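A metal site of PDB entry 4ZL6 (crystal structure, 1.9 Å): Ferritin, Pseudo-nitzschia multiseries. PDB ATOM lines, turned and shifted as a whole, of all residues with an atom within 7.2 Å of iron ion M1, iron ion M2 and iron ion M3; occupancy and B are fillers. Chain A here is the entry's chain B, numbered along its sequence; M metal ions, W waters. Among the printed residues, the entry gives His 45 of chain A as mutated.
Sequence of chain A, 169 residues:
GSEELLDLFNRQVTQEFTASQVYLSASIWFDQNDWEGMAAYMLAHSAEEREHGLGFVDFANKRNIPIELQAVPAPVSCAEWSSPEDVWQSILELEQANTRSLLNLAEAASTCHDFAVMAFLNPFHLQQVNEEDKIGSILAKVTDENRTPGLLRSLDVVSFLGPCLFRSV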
ATOM      1  N   GLN A  12     -19.253 -20.013  -3.408  1.00  0.00           N
ATOM      2  CA  GLN A  12     -20.566 -20.446  -3.806  1.00  0.00           C
ATOM      3  C   GLN A  12     -20.638 -21.960  -3.913  1.00  0.00           C
ATOM      4  O   GLN A  12     -21.664 -22.550  -3.573  1.00  0.00           O
ATOM      5  CB  GLN A  12     -20.962 -19.817  -5.139  1.00  0.00           C
ATOM      6  CG  GLN A  12     -22.401 -20.038  -5.522  1.00  0.00           C
ATOM      7  CD  GLN A  12     -23.304 -19.353  -4.517  1.00  0.00           C
ATOM      8  OE1 GLN A  12     -22.989 -18.266  -3.963  1.00  0.00           O
ATOM      9  NE2 GLN A  12     -24.392 -19.992  -4.224  1.00  0.00           N
ATOM     10  N   GLN A  15     -21.088 -23.121  -0.509  1.00  0.00           N
ATOM     11  CA  GLN A  15     -22.440 -22.853  -0.067  1.00  0.00           C
ATOM     12  C   GLN A  15     -23.415 -23.933  -0.558  1.00  0.00           C
ATOM     13  O   GLN A  15     -24.263 -24.349   0.219  1.00  0.00           O
ATOM     14  CB  GLN A  15     -22.959 -21.426  -0.398  1.00  0.00           C
ATOM     15  CG  GLN A  15     -22.318 -20.372   0.503  1.00  0.00           C
ATOM     16  CD  GLN A  15     -22.465 -20.779   1.962  1.00  0.00           C
ATOM     17  OE1 GLN A  15     -23.601 -20.850   2.440  1.00  0.00           O
ATOM     18  NE2 GLN A  15     -21.323 -21.244   2.619  1.00  0.00           N
ATOM     19  N   GLU A  16     -23.313 -24.326  -1.842  1.00  0.00           N
ATOM     20  CA  GLU A  16     -24.215 -25.335  -2.393  1.00  0.00           C
ATOM     21  C   GLU A  16     -24.024 -26.711  -1.741  1.00  0.00           C
ATOM     22  O   GLU A  16     -25.017 -27.345  -1.376  1.00  0.00           O
ATOM     23  CB  GLU A  16     -23.979 -25.485  -3.867  1.00  0.00           C
ATOM     24  CG  GLU A  16     -24.257 -24.283  -4.716  1.00  0.00           C
ATOM     25  CD  GLU A  16     -25.664 -23.714  -4.584  1.00  0.00           C
ATOM     26  OE1 GLU A  16     -26.630 -24.453  -4.301  1.00  0.00           O
ATOM     27  OE2 GLU A  16     -25.783 -22.500  -4.818  1.00  0.00           O
ATOM     28  N   ALA A  19     -25.424 -26.481   1.761  1.00  0.00           N
ATOM     29  CA  ALA A  19     -26.876 -26.616   1.704  1.00  0.00           C
ATOM     30  C   ALA A  19     -27.263 -28.057   1.413  1.00  0.00           C
ATOM     31  O   ALA A  19     -28.218 -28.577   2.013  1.00  0.00           O
ATOM     32  CB  ALA A  19     -27.491 -25.643   0.665  1.00  0.00           C
ATOM     33  N   SER A  20     -26.489 -28.773   0.573  1.00  0.00           N
ATOM     34  CA  SER A  20     -26.818 -30.158   0.347  1.00  0.00           C
ATOM     35  C   SER A  20     -26.841 -30.998   1.653  1.00  0.00           C
ATOM     36  O   SER A  20     -27.761 -31.839   1.902  1.00  0.00           O
ATOM     37  CB  SER A  20     -25.827 -30.736  -0.688  1.00  0.00           C
ATOM     38  OG  SER A  20     -26.138 -32.037  -0.914  1.00  0.00           O
ATOM     39  N   TYR A  23     -29.890 -30.023   3.918  1.00  0.00           N
ATOM     40  CA  TYR A  23     -31.074 -30.717   3.427  1.00  0.00           C
ATOM     41  C   TYR A  23     -31.040 -32.189   3.823  1.00  0.00           C
ATOM     42  O   TYR A  23     -32.078 -32.746   4.256  1.00  0.00           O
ATOM     43  CB  TYR A  23     -31.234 -30.578   1.890  1.00  0.00           C
ATOM     44  CG  TYR A  23     -31.961 -29.355   1.441  1.00  0.00           C
ATOM     45  CD1 TYR A  23     -33.340 -29.260   1.564  1.00  0.00           C
ATOM     46  CD2 TYR A  23     -31.286 -28.291   0.879  1.00  0.00           C
ATOM     47  CE1 TYR A  23     -34.059 -28.146   1.131  1.00  0.00           C
ATOM     48  CE2 TYR A  23     -31.984 -27.138   0.521  1.00  0.00           C
ATOM     49  CZ  TYR A  23     -33.345 -27.104   0.597  1.00  0.00           C
ATOM     50  OH  TYR A  23     -34.003 -26.025   0.158  1.00  0.00           O
ATOM     51  N   TYR A  41     -38.865 -35.170   0.224  1.00  0.00           N
ATOM     52  CA  TYR A  41     -38.672 -33.885  -0.388  1.00  0.00           C
ATOM     53  C   TYR A  41     -37.255 -33.323  -0.036  1.00  0.00           C
ATOM     54  O   TYR A  41     -36.517 -32.821  -0.895  1.00  0.00           O
ATOM     55  CB  TYR A  41     -39.730 -32.906   0.069  1.00  0.00           C
ATOM     56  CG  TYR A  41     -39.482 -31.520  -0.355  1.00  0.00           C
ATOM     57  CD1 TYR A  41     -38.660 -30.706   0.399  1.00  0.00           C
ATOM     58  CD2 TYR A  41     -40.009 -31.026  -1.533  1.00  0.00           C
ATOM     59  CE1 TYR A  41     -38.362 -29.440   0.004  1.00  0.00           C
ATOM     60  CE2 TYR A  41     -39.733 -29.724  -1.936  1.00  0.00           C
ATOM     61  CZ  TYR A  41     -38.918 -28.947  -1.179  1.00  0.00           C
ATOM     62  OH  TYR A  41     -38.574 -27.694  -1.546  1.00  0.00           O
ATOM     63  N   HIS A  45     -34.095 -32.488  -2.616  1.00  0.00           N
ATOM     64  CA  HIS A  45     -33.563 -31.167  -2.698  1.00  0.00           C
ATOM     65  C   HIS A  45     -32.038 -31.232  -2.327  1.00  0.00           C
ATOM     66  O   HIS A  45     -31.250 -30.510  -2.884  1.00  0.00           O
ATOM     67  CB  HIS A  45     -34.317 -30.230  -1.773  1.00  0.00           C
ATOM     68  CG  HIS A  45     -34.242 -28.808  -2.203  1.00  0.00           C
ATOM     69  ND1 HIS A  45     -35.369 -28.031  -2.382  1.00  0.00           N
ATOM     70  CD2 HIS A  45     -33.182 -28.048  -2.609  1.00  0.00           C
ATOM     71  CE1 HIS A  45     -34.993 -26.815  -2.761  1.00  0.00           C
ATOM     72  NE2 HIS A  45     -33.680 -26.827  -2.968  1.00  0.00           N
ATOM     73  N   GLU A  48     -30.313 -32.014  -5.488  1.00  0.00           N
ATOM     74  CA  GLU A  48     -30.378 -30.864  -6.349  1.00  0.00           C
ATOM     75  C   GLU A  48     -29.355 -29.783  -5.960  1.00  0.00           C
ATOM     76  O   GLU A  48     -28.733 -29.149  -6.845  1.00  0.00           O
ATOM     77  CB  GLU A  48     -31.797 -30.236  -6.279  1.00  0.00           C
ATOM     78  CG  GLU A  48     -31.802 -28.920  -7.033  1.00  0.00           C
ATOM     79  CD  GLU A  48     -33.202 -28.368  -7.281  1.00  0.00           C
ATOM     80  OE1 GLU A  48     -33.956 -28.142  -6.289  1.00  0.00           O
ATOM     81  OE2 GLU A  48     -33.509 -28.127  -8.470  1.00  0.00           O
ATOM     82  N   GLU A  49     -29.167 -29.561  -4.654  1.00  0.00           N
ATOM     83  CA  GLU A  49     -28.154 -28.575  -4.270  1.00  0.00           C
ATOM     84  C   GLU A  49     -26.744 -29.052  -4.708  1.00  0.00           C
ATOM     85  O   GLU A  49     -25.889 -28.289  -5.091  1.00  0.00           O
ATOM     86  CB  GLU A  49     -28.076 -28.416  -2.780  1.00  0.00           C
ATOM     87  CG  GLU A  49     -29.326 -27.901  -2.204  1.00  0.00           C
ATOM     88  CD  GLU A  49     -29.653 -26.480  -2.637  1.00  0.00           C
ATOM     89  OE1 GLU A  49     -28.872 -25.694  -3.134  1.00  0.00           O
ATOM     90  OE2 GLU A  49     -30.712 -26.123  -2.319  1.00  0.00           O
ATOM     91  N   ARG A  50     -26.514 -30.342  -4.552  1.00  0.00           N
ATOM     92  CA  ARG A  50     -25.243 -30.910  -5.001  1.00  0.00           C
ATOM     93  C   ARG A  50     -25.083 -30.673  -6.494  1.00  0.00           C
ATOM     94  O   ARG A  50     -23.996 -30.281  -6.967  1.00  0.00           O
ATOM     95  CB  ARG A  50     -25.139 -32.391  -4.709  1.00  0.00           C
ATOM     96  CG  ARG A  50     -23.742 -32.947  -5.026  1.00  0.00           C
ATOM     97  CD  ARG A  50     -23.395 -34.250  -4.297  1.00  0.00           C
ATOM     98  NE  ARG A  50     -22.168 -34.853  -4.850  1.00  0.00           N
ATOM     99  CZ  ARG A  50     -22.161 -35.493  -6.034  1.00  0.00           C
ATOM    100  NH1 ARG A  50     -23.236 -35.646  -6.762  1.00  0.00           N
ATOM    101  NH2 ARG A  50     -21.039 -35.898  -6.529  1.00  0.00           N
ATOM    102  N   HIS A  52     -26.275 -28.192  -8.309  1.00  0.00           N
ATOM    103  CA  HIS A  52     -25.883 -26.817  -8.422  1.00  0.00           C
ATOM    104  C   HIS A  52     -24.412 -26.584  -8.170  1.00  0.00           C
ATOM    105  O   HIS A  52     -23.723 -25.885  -8.969  1.00  0.00           O
ATOM    106  CB  HIS A  52     -26.633 -25.882  -7.484  1.00  0.00           C
ATOM    107  CG  HIS A  52     -28.099 -25.900  -7.684  1.00  0.00           C
ATOM    108  ND1 HIS A  52     -28.668 -26.268  -8.881  1.00  0.00           N
ATOM    109  CD2 HIS A  52     -29.118 -25.614  -6.827  1.00  0.00           C
ATOM    110  CE1 HIS A  52     -29.988 -26.210  -8.763  1.00  0.00           C
ATOM    111  NE2 HIS A  52     -30.280 -25.805  -7.545  1.00  0.00           N
ATOM    112  N   GLY A  53     -23.887 -27.141  -7.087  1.00  0.00           N
ATOM    113  CA  GLY A  53     -22.479 -27.006  -6.906  1.00  0.00           C
ATOM    114  C   GLY A  53     -21.640 -27.578  -8.051  1.00  0.00           C
ATOM    115  O   GLY A  53     -20.657 -26.988  -8.466  1.00  0.00           O
ATOM    116  N   PHE A  56     -21.502 -25.131 -10.893  1.00  0.00           N
ATOM    117  CA  PHE A  56     -20.527 -24.094 -10.661  1.00  0.00           C
ATOM    118  C   PHE A  56     -19.149 -24.602 -10.926  1.00  0.00           C
ATOM    119  O   PHE A  56     -18.320 -23.871 -11.511  1.00  0.00           O
ATOM    120  CB  PHE A  56     -20.647 -23.526  -9.280  1.00  0.00           C
ATOM    121  CG  PHE A  56     -21.752 -22.457  -9.172  1.00  0.00           C
ATOM    122  CD1 PHE A  56     -23.086 -22.808  -9.167  1.00  0.00           C
ATOM    123  CD2 PHE A  56     -21.447 -21.117  -9.198  1.00  0.00           C
ATOM    124  CE1 PHE A  56     -24.111 -21.873  -9.150  1.00  0.00           C
ATOM    125  CE2 PHE A  56     -22.477 -20.157  -9.160  1.00  0.00           C
ATOM    126  CZ  PHE A  56     -23.794 -20.542  -9.158  1.00  0.00           C
ATOM    127  N   LEU A  94     -31.882 -21.001   4.938  1.00  0.00           N
ATOM    128  CA  LEU A  94     -30.768 -21.533   4.164  1.00  0.00           C
ATOM    129  C   LEU A  94     -30.904 -21.024   2.737  1.00  0.00           C
ATOM    130  O   LEU A  94     -29.937 -20.601   2.092  1.00  0.00           O
ATOM    131  CB  LEU A  94     -30.866 -23.068   4.239  1.00  0.00           C
ATOM    132  CG  LEU A  94     -29.857 -23.867   3.427  1.00  0.00           C
ATOM    133  CD1 LEU A  94     -28.484 -23.748   4.031  1.00  0.00           C
ATOM    134  CD2 LEU A  94     -30.269 -25.296   3.270  1.00  0.00           C
ATOM    135  N   GLU A  95     -32.105 -21.125   2.172  1.00  0.00           N
ATOM    136  CA  GLU A  95     -32.316 -20.605   0.835  1.00  0.00           C
ATOM    137  C   GLU A  95     -32.173 -19.112   0.721  1.00  0.00           C
ATOM    138  O   GLU A  95     -31.621 -18.604  -0.267  1.00  0.00           O
ATOM    139  CB  GLU A  95     -33.634 -21.106   0.244  1.00  0.00           C
ATOM    140  CG  GLU A  95     -33.654 -22.603  -0.071  1.00  0.00           C
ATOM    141  CD  GLU A  95     -32.783 -23.048  -1.221  1.00  0.00           C
ATOM    142  OE1 GLU A  95     -32.165 -22.202  -1.899  1.00  0.00           O
ATOM    143  OE2 GLU A  95     -32.733 -24.281  -1.470  1.00  0.00           O
ATOM    144  N   ASN A  98     -28.549 -18.695   0.495  1.00  0.00           N
ATOM    145  CA  ASN A  98     -28.071 -19.129  -0.828  1.00  0.00           C
ATOM    146  C   ASN A  98     -28.334 -17.895  -1.799  1.00  0.00           C
ATOM    147  O   ASN A  98     -27.489 -17.510  -2.596  1.00  0.00           O
ATOM    148  CB  ASN A  98     -28.795 -20.398  -1.430  1.00  0.00           C
ATOM    149  CG  ASN A  98     -28.471 -21.814  -0.788  1.00  0.00           C
ATOM    150  OD1 ASN A  98     -27.508 -22.010  -0.041  1.00  0.00           O
ATOM    151  ND2 ASN A  98     -29.305 -22.855  -1.156  1.00  0.00           N
ATOM    152  N   LEU A 102     -25.586 -15.658  -3.966  1.00  0.00           N
ATOM    153  CA  LEU A 102     -25.619 -15.537  -5.446  1.00  0.00           C
ATOM    154  C   LEU A 102     -25.601 -14.114  -5.877  1.00  0.00           C
ATOM    155  O   LEU A 102     -24.986 -13.741  -6.904  1.00  0.00           O
ATOM    156  CB  LEU A 102     -26.858 -16.197  -6.041  1.00  0.00           C
ATOM    157  CG  LEU A 102     -26.786 -17.676  -6.234  1.00  0.00           C
ATOM    158  CD1 LEU A 102     -28.196 -18.113  -6.650  1.00  0.00           C
ATOM    159  CD2 LEU A 102     -25.781 -18.055  -7.307  1.00  0.00           C
ATOM    160  N   PHE A 124     -29.907 -19.276 -12.316  1.00  0.00           N
ATOM    161  CA  PHE A 124     -29.875 -19.497 -10.891  1.00  0.00           C
ATOM    162  C   PHE A 124     -30.605 -18.358 -10.139  1.00  0.00           C
ATOM    163  O   PHE A 124     -31.235 -18.623  -9.096  1.00  0.00           O
ATOM    164  CB  PHE A 124     -28.431 -19.552 -10.398  1.00  0.00           C
ATOM    165  CG  PHE A 124     -27.662 -20.727 -10.926  1.00  0.00           C
ATOM    166  CD1 PHE A 124     -27.776 -21.957 -10.288  1.00  0.00           C
ATOM    167  CD2 PHE A 124     -26.856 -20.628 -12.072  1.00  0.00           C
ATOM    168  CE1 PHE A 124     -27.085 -23.073 -10.793  1.00  0.00           C
ATOM    169  CE2 PHE A 124     -26.168 -21.745 -12.598  1.00  0.00           C
ATOM    170  CZ  PHE A 124     -26.304 -22.953 -11.964  1.00  0.00           C
ATOM    171  N   GLN A 127     -34.238 -19.439 -10.545  1.00  0.00           N
ATOM    172  CA  GLN A 127     -34.507 -20.615  -9.741  1.00  0.00           C
ATOM    173  C   GLN A 127     -34.646 -20.254  -8.251  1.00  0.00           C
ATOM    174  O   GLN A 127     -35.567 -20.799  -7.599  1.00  0.00           O
ATOM    175  CB  GLN A 127     -33.394 -21.674  -9.895  1.00  0.00           C
ATOM    176  CG  GLN A 127     -33.573 -22.862  -8.912  1.00  0.00           C
ATOM    177  CD  GLN A 127     -33.090 -24.235  -9.446  1.00  0.00           C
ATOM    178  OE1 GLN A 127     -33.251 -25.256  -8.754  1.00  0.00           O
ATOM    179  NE2 GLN A 127     -32.497 -24.263 -10.656  1.00  0.00           N
ATOM    180  N   GLN A 128     -33.768 -19.418  -7.728  1.00  0.00           N
ATOM    181  CA  GLN A 128     -33.837 -19.031  -6.313  1.00  0.00           C
ATOM    182  C   GLN A 128     -35.185 -18.355  -6.016  1.00  0.00           C
ATOM    183  O   GLN A 128     -35.763 -18.580  -4.946  1.00  0.00           O
ATOM    184  CB  GLN A 128     -32.691 -18.139  -5.849  1.00  0.00           C
ATOM    185  CG  GLN A 128     -31.393 -18.885  -5.704  1.00  0.00           C
ATOM    186  CD  GLN A 128     -31.552 -20.058  -4.757  1.00  0.00           C
ATOM    187  OE1 GLN A 128     -31.581 -21.228  -5.172  1.00  0.00           O
ATOM    188  NE2 GLN A 128     -31.820 -19.743  -3.494  1.00  0.00           N
ATOM    189  N   GLU A 131     -37.686 -21.195  -5.711  1.00  0.00           N
ATOM    190  CA  GLU A 131     -37.462 -22.008  -4.500  1.00  0.00           C
ATOM    191  C   GLU A 131     -37.880 -21.326  -3.240  1.00  0.00           C
ATOM    192  O   GLU A 131     -38.534 -21.969  -2.413  1.00  0.00           O
ATOM    193  CB  GLU A 131     -35.990 -22.431  -4.394  1.00  0.00           C
ATOM    194  CG  GLU A 131     -35.750 -23.492  -5.424  1.00  0.00           C
ATOM    195  CD  GLU A 131     -34.363 -24.078  -5.331  1.00  0.00           C
ATOM    196  OE1 GLU A 131     -33.767 -23.904  -4.276  1.00  0.00           O
ATOM    197  OE2 GLU A 131     -33.925 -24.664  -6.329  1.00  0.00           O
ATOM    198  N   ILE A 135     -40.777 -22.823  -0.850  1.00  0.00           N
ATOM    199  CA  ILE A 135     -40.444 -23.183   0.530  1.00  0.00           C
ATOM    200  C   ILE A 135     -41.305 -22.352   1.468  1.00  0.00           C
ATOM    201  O   ILE A 135     -41.912 -22.885   2.411  1.00  0.00           O
ATOM    202  CB  ILE A 135     -38.974 -22.962   0.863  1.00  0.00           C
ATOM    203  CG1 ILE A 135     -38.088 -23.877   0.000  1.00  0.00           C
ATOM    204  CG2 ILE A 135     -38.736 -23.197   2.347  1.00  0.00           C
ATOM    205  CD1 ILE A 135     -38.220 -25.344   0.283  1.00  0.00           C
HETATM  206 FE    FE M   1     -32.189 -25.073  -3.422  1.00  0.00          FE
HETATM  207 FE    FE M   2     -32.021 -24.984  -6.947  1.00  0.00          FE
HETATM  208 FE    FE M   3     -28.726 -24.075  -4.335  1.00  0.00          FE
HETATM  209  O   HOH W   1     -30.893 -23.368  -3.973  1.00  0.00           O
HETATM  210  O   HOH W   2     -28.373 -22.215  -5.656  1.00  0.00           O
HETATM  211  O   HOH W   3     -31.944 -26.228  -5.121  1.00  0.00           O
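Merely in contact with iron ion M2: Glu 48 (3.6 Å).
Of the 23 residues printed, 4 come within 4 Å of iron ion M2.
The nearest printed residue that does not touch iron ion M2 is Gln 128 (4.2 Å).
Water W1 lies within hydrogen-bond range of the side-chain amide oxygen of Gln 128, the side-chain carboxylate of Glu 95 and the side-chain amide nitrogen of Asn 98.
Water W2 lies within hydrogen-bond range of the side-chain carboxylate (OE2) of Glu 16 (2.7 Å) and the side-chain amide oxygen (OE1) of Gln 128 (3.4 Å).
Iron ion M2 is bound by NE2 of His 52 (2.0 Å), OE2 of Glu 131 (2.0 Å), OE1 of Gln 127 (2.2 Å) and water W3 (2.2 Å).
Iron ion M2 has four donor atoms within binding distance.
Residues that only touch iron ion M3: Asn 98 (3.5 Å).
Four residues have an atom within 4 Å of iron ion M3: Glu 16, Glu 49, His 52 and Asn 98.
Iron ion M3 is bound by the side-chain carboxylate of Glu 49 (2.0 Å), the side-chain carboxylate of Glu 16 (2.1 Å), water W2 (2.3 Å) and water W1 (2.3 Å).
Iron ion M3 has four donor atoms within binding distance.
Iron ion M1 is bound by water W3 (2.1 Å), OE2 of Glu 49 (2.1 Å), OE1 of Glu 131 (2.1 Å), OE2 of Glu 95 (2.2 Å), water W1 (2.2 Å) and NE2 of His 45 (2.3 Å).
Four residues have an atom within 4 Å of iron ion M1: His 45, Glu 49, Glu 95 and Glu 131.
The side-chain amide nitrogen of Asn 98 lies close to the side-chain carboxylate of Glu 49, at 3.5 Å.
The side-chain carboxylate (OE2) of Glu 16 lies within hydrogen-bond range of the side-chain amide nitrogen (NE2) of Gln 12, at 2.9 Å.
The side-chain carboxylate of Glu 95 is in hydrogen-bond range of the side-chain amide nitrogen of Asn 98, at 3.0 Å.
The side-chain carboxylate (OE1) of Glu 95 lies within hydrogen-bond range of the side-chain amide nitrogen (NE2) of Gln 128.
The side-chain carboxylate (OE2) of Glu 95 sits close to the side-chain hydroxyl (OH) of Tyr 23, at 2.7 Å.
The side-chain amide oxygen (OE1) of Gln 127 sits close to the side-chain carboxylate (OE2) of Glu 48.
The side-chain hydroxyl (OH) of Tyr 23 sits close to a ring nitrogen (NE2) of His 45 (3.2 Å).
The side-chain hydroxyl (OH) of Tyr 41 is in hydrogen-bond range of a ring nitrogen (ND1) of His 45, 3.3 Å away.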
